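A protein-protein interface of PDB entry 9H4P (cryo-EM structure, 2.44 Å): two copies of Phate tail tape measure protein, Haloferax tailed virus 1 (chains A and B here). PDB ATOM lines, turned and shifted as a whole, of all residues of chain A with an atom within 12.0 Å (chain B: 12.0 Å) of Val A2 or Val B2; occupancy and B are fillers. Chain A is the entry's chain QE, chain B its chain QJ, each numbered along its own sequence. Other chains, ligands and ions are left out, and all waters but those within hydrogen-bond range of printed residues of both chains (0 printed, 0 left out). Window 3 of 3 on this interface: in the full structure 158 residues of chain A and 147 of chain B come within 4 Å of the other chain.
Val A2 touches its own counterpart, Val B2.
Ile A4 touches Val B2, but with the chains exchanged Val A2 does not touch Ile B4 (9.3 Å).
Arg A5 touches Val B9, but with the chains exchanged Val A9 does not touch Arg B5 (9.5 Å).
Gly A8 touches Ser B10, but with the chains exchanged Ser A10 does not touch Gly B8 (10.6 Å).
Positions printed for both chains: 2, 3, 4, 5, 6, 7, 8, 9 and 10.
Of the 9 printed residues of chain A, 5 touch a printed residue of chain B.
Along chain A the printed residues that touch a printed residue of chain B span positions 2 to 9.
Among the printed residues, no Asp or Glu carboxylate lies within 4 Å of a Lys or Arg side-chain nitrogen of the other chain.
Val A2 touches one residue of chain B.
Of chain A, only Val A2 and Ile A4 come within 4 Å of Val B2.
Of chain B, only Val B2 and Ser B6 come within 4 Å of Ile A4.
Ile B4 touches none of the printed residues of chain A.
Ser B6 touches just one residue of chain A: Ile A4 (3.4 Å).
Printed residues of chain B within 4 Å of Gly A8: Val B9 and Ser B10.
Printed residues of chain B within 4 Å of Val A9: Val B9.
Of the printed residues of chain A, Ser B10 touches Gly A8 (3.2 Å).
Glu A7 touches none of the printed residues of chain B.
Ser A10 touches none of the printed residues of chain B.
The nearest printed residue of chain A that does not touch Val B9 is Ile A4 (6.0 Å).
Among the printed residues, merely in contact across the chains: Gly A8 with Ser B10, Ile A4 with Ser B6, Ile A4 with Val B2, Val A2 with Val B2, Val A9 with Val B9, Gly A8 with Val B9 and Arg A5 with Val B9.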
ATOM      1  N   VAL A   2      -0.898  -2.479   2.059  1.00  0.00           N
ATOM      2  CA  VAL A   2       0.495  -2.683   2.539  1.00  0.00           C
ATOM      3  C   VAL A   2       0.525  -3.938   3.411  1.00  0.00           C
ATOM      4  O   VAL A   2      -0.306  -4.081   4.303  1.00  0.00           O
ATOM      5  CB  VAL A   2       1.019  -1.437   3.281  1.00  0.00           C
ATOM      6  CG1 VAL A   2       2.333  -1.701   3.994  1.00  0.00           C
ATOM      7  CG2 VAL A   2       1.155  -0.245   2.352  1.00  0.00           C
ATOM      8  N   ALA A   3       1.480  -4.845   3.144  1.00  0.00           N
ATOM      9  CA  ALA A   3       1.632  -6.073   3.915  1.00  0.00           C
ATOM     10  C   ALA A   3       3.105  -6.448   4.128  1.00  0.00           C
ATOM     11  O   ALA A   3       3.439  -7.627   4.230  1.00  0.00           O
ATOM     12  CB  ALA A   3       0.839  -7.182   3.269  1.00  0.00           C
ATOM     13  N   ILE A   4       3.966  -5.430   4.259  1.00  0.00           N
ATOM     14  CA  ILE A   4       5.420  -5.532   4.310  1.00  0.00           C
ATOM     15  C   ILE A   4       5.917  -6.371   5.494  1.00  0.00           C
ATOM     16  O   ILE A   4       6.902  -7.088   5.344  1.00  0.00           O
ATOM     17  CB  ILE A   4       6.061  -4.130   4.187  1.00  0.00           C
ATOM     18  CG1 ILE A   4       6.145  -3.710   2.719  1.00  0.00           C
ATOM     19  CG2 ILE A   4       7.429  -4.071   4.845  1.00  0.00           C
ATOM     20  CD1 ILE A   4       6.638  -2.306   2.481  1.00  0.00           C
ATOM     21  N   ARG A   5       5.233  -6.317   6.647  1.00  0.00           N
ATOM     22  CA  ARG A   5       5.617  -7.119   7.805  1.00  0.00           C
ATOM     23  C   ARG A   5       5.059  -8.542   7.742  1.00  0.00           C
ATOM     24  O   ARG A   5       5.792  -9.478   8.042  1.00  0.00           O
ATOM     25  CB  ARG A   5       5.286  -6.443   9.141  1.00  0.00           C
ATOM     26  CG  ARG A   5       5.924  -7.122  10.347  1.00  0.00           C
ATOM     27  CD  ARG A   5       5.661  -6.454  11.679  1.00  0.00           C
ATOM     28  NE  ARG A   5       6.392  -7.071  12.778  1.00  0.00           N
ATOM     29  CZ  ARG A   5       5.965  -8.087  13.517  1.00  0.00           C
ATOM     30  NH1 ARG A   5       6.729  -8.553  14.487  1.00  0.00           N
ATOM     31  NH2 ARG A   5       4.790  -8.642  13.292  1.00  0.00           N
ATOM     32  N   SER A   6       3.780  -8.714   7.380  1.00  0.00           N
ATOM     33  CA  SER A   6       3.100  -9.991   7.556  1.00  0.00           C
ATOM     34  C   SER A   6       3.698 -11.106   6.696  1.00  0.00           C
ATOM     35  O   SER A   6       3.677 -12.263   7.106  1.00  0.00           O
ATOM     36  CB  SER A   6       1.619  -9.866   7.361  1.00  0.00           C
ATOM     37  OG  SER A   6       1.313  -9.483   6.033  1.00  0.00           O
ATOM     38  N   GLU A   7       4.231 -10.753   5.521  1.00  0.00           N
ATOM     39  CA  GLU A   7       4.789 -11.705   4.568  1.00  0.00           C
ATOM     40  C   GLU A   7       6.067 -12.355   5.103  1.00  0.00           C
ATOM     41  O   GLU A   7       6.322 -13.524   4.827  1.00  0.00           O
ATOM     42  CB  GLU A   7       4.969 -11.073   3.183  1.00  0.00           C
ATOM     43  CG  GLU A   7       5.966  -9.926   3.116  1.00  0.00           C
ATOM     44  CD  GLU A   7       6.107  -9.219   1.778  1.00  0.00           C
ATOM     45  OE1 GLU A   7       5.413  -9.595   0.826  1.00  0.00           O
ATOM     46  OE2 GLU A   7       6.924  -8.289   1.694  1.00  0.00           O
ATOM     47  N   GLY A   8       6.857 -11.599   5.871  1.00  0.00           N
ATOM     48  CA  GLY A   8       8.147 -12.056   6.363  1.00  0.00           C
ATOM     49  C   GLY A   8       8.047 -12.938   7.606  1.00  0.00           C
ATOM     50  O   GLY A   8       8.859 -13.843   7.780  1.00  0.00           O
ATOM     51  N   VAL A   9       7.051 -12.673   8.463  1.00  0.00           N
ATOM     52  CA  VAL A   9       6.885 -13.407   9.711  1.00  0.00           C
ATOM     53  C   VAL A   9       6.061 -14.680   9.511  1.00  0.00           C
ATOM     54  O   VAL A   9       6.412 -15.715  10.070  1.00  0.00           O
ATOM     55  CB  VAL A   9       6.360 -12.529  10.866  1.00  0.00           C
ATOM     56  CG1 VAL A   9       4.966 -11.979  10.622  1.00  0.00           C
ATOM     57  CG2 VAL A   9       6.427 -13.235  12.209  1.00  0.00           C
ATOM     58  N   SER A  10       4.980 -14.619   8.718  1.00  0.00           N
ATOM     59  CA  SER A  10       4.011 -15.707   8.673  1.00  0.00           C
ATOM     60  C   SER A  10       4.554 -16.982   8.019  1.00  0.00           C
ATOM     61  O   SER A  10       3.938 -18.036   8.169  1.00  0.00           O
ATOM     62  CB  SER A  10       2.675 -15.284   8.122  1.00  0.00           C
ATOM     63  OG  SER A  10       2.801 -14.736   6.824  1.00  0.00           O
ATOM     64  N   VAL B   2       5.721   2.406   7.931  1.00  0.00           N
ATOM     65  CA  VAL B   2       5.653   1.149   7.147  1.00  0.00           C
ATOM     66  C   VAL B   2       6.979   0.395   7.286  1.00  0.00           C
ATOM     67  O   VAL B   2       6.990  -0.667   7.896  1.00  0.00           O
ATOM     68  CB  VAL B   2       5.225   1.395   5.686  1.00  0.00           C
ATOM     69  CG1 VAL B   2       5.377   0.145   4.845  1.00  0.00           C
ATOM     70  CG2 VAL B   2       3.798   1.912   5.599  1.00  0.00           C
ATOM     71  N   ALA B   3       8.091   0.946   6.771  1.00  0.00           N
ATOM     72  CA  ALA B   3       9.342   0.207   6.616  1.00  0.00           C
ATOM     73  C   ALA B   3      10.332   0.409   7.774  1.00  0.00           C
ATOM     74  O   ALA B   3      11.529   0.207   7.589  1.00  0.00           O
ATOM     75  CB  ALA B   3       9.956   0.529   5.276  1.00  0.00           C
ATOM     76  N   ILE B   4       9.846   0.732   8.982  1.00  0.00           N
ATOM     77  CA  ILE B   4      10.683   1.213  10.080  1.00  0.00           C
ATOM     78  C   ILE B   4      11.561   0.111  10.693  1.00  0.00           C
ATOM     79  O   ILE B   4      12.727   0.369  10.987  1.00  0.00           O
ATOM     80  CB  ILE B   4       9.861   2.011  11.119  1.00  0.00           C
ATOM     81  CG1 ILE B   4      10.753   2.762  12.111  1.00  0.00           C
ATOM     82  CG2 ILE B   4       8.830   1.140  11.820  1.00  0.00           C
ATOM     83  CD1 ILE B   4      10.045   3.835  12.903  1.00  0.00           C
ATOM     84  N   ARG B   5      11.013  -1.106  10.884  1.00  0.00           N
ATOM     85  CA  ARG B   5      11.718  -2.236  11.492  1.00  0.00           C
ATOM     86  C   ARG B   5      11.424  -3.569  10.787  1.00  0.00           C
ATOM     87  O   ARG B   5      11.669  -4.630  11.358  1.00  0.00           O
ATOM     88  CB  ARG B   5      11.453  -2.329  13.002  1.00  0.00           C
ATOM     89  CG  ARG B   5      11.967  -1.155  13.824  1.00  0.00           C
ATOM     90  CD  ARG B   5      12.119  -1.421  15.309  1.00  0.00           C
ATOM     91  NE  ARG B   5      10.891  -1.844  15.964  1.00  0.00           N
ATOM     92  CZ  ARG B   5      10.707  -1.932  17.275  1.00  0.00           C
ATOM     93  NH1 ARG B   5       9.542  -2.335  17.747  1.00  0.00           N
ATOM     94  NH2 ARG B   5      11.674  -1.615  18.112  1.00  0.00           N
ATOM     95  N   SER B   6      10.952  -3.509   9.532  1.00  0.00           N
ATOM     96  CA  SER B   6      10.568  -4.669   8.738  1.00  0.00           C
ATOM     97  C   SER B   6      11.749  -5.368   8.054  1.00  0.00           C
ATOM     98  O   SER B   6      11.606  -6.522   7.662  1.00  0.00           O
ATOM     99  CB  SER B   6       9.526  -4.281   7.731  1.00  0.00           C
ATOM    100  OG  SER B   6      10.008  -3.250   6.884  1.00  0.00           O
ATOM    101  N   GLU B   7      12.907  -4.702   7.920  1.00  0.00           N
ATOM    102  CA  GLU B   7      14.008  -5.139   7.064  1.00  0.00           C
ATOM    103  C   GLU B   7      14.710  -6.414   7.545  1.00  0.00           C
ATOM    104  O   GLU B   7      15.522  -6.966   6.805  1.00  0.00           O
ATOM    105  CB  GLU B   7      15.041  -4.023   6.898  1.00  0.00           C
ATOM    106  CG  GLU B   7      14.668  -2.974   5.869  1.00  0.00           C
ATOM    107  CD  GLU B   7      15.851  -2.476   5.063  1.00  0.00           C
ATOM    108  OE1 GLU B   7      16.198  -3.127   4.064  1.00  0.00           O
ATOM    109  OE2 GLU B   7      16.430  -1.453   5.452  1.00  0.00           O
ATOM    110  N   GLY B   8      14.407  -6.881   8.765  1.00  0.00           N
ATOM    111  CA  GLY B   8      15.006  -8.088   9.322  1.00  0.00           C
ATOM    112  C   GLY B   8      14.000  -9.126   9.822  1.00  0.00           C
ATOM    113  O   GLY B   8      14.407 -10.121  10.416  1.00  0.00           O
ATOM    114  N   VAL B   9      12.705  -8.906   9.565  1.00  0.00           N
ATOM    115  CA  VAL B   9      11.637  -9.764  10.065  1.00  0.00           C
ATOM    116  C   VAL B   9      11.706 -11.156   9.433  1.00  0.00           C
ATOM    117  O   VAL B   9      11.554 -12.146  10.144  1.00  0.00           O
ATOM    118  CB  VAL B   9      10.251  -9.101   9.931  1.00  0.00           C
ATOM    119  CG1 VAL B   9       9.110 -10.067  10.191  1.00  0.00           C
ATOM    120  CG2 VAL B   9      10.126  -7.907  10.858  1.00  0.00           C
ATOM    121  N   SER B  10      11.958 -11.234   8.118  1.00  0.00           N
ATOM    122  CA  SER B  10      12.017 -12.514   7.423  1.00  0.00           C
ATOM    123  C   SER B  10      13.236 -13.335   7.838  1.00  0.00           C
ATOM    124  O   SER B  10      13.239 -14.543   7.631  1.00  0.00           O
ATOM    125  CB  SER B  10      11.939 -12.385   5.924  1.00  0.00           C
ATOM    126  OG  SER B  10      11.113 -11.305   5.531  1.00  0.00           O
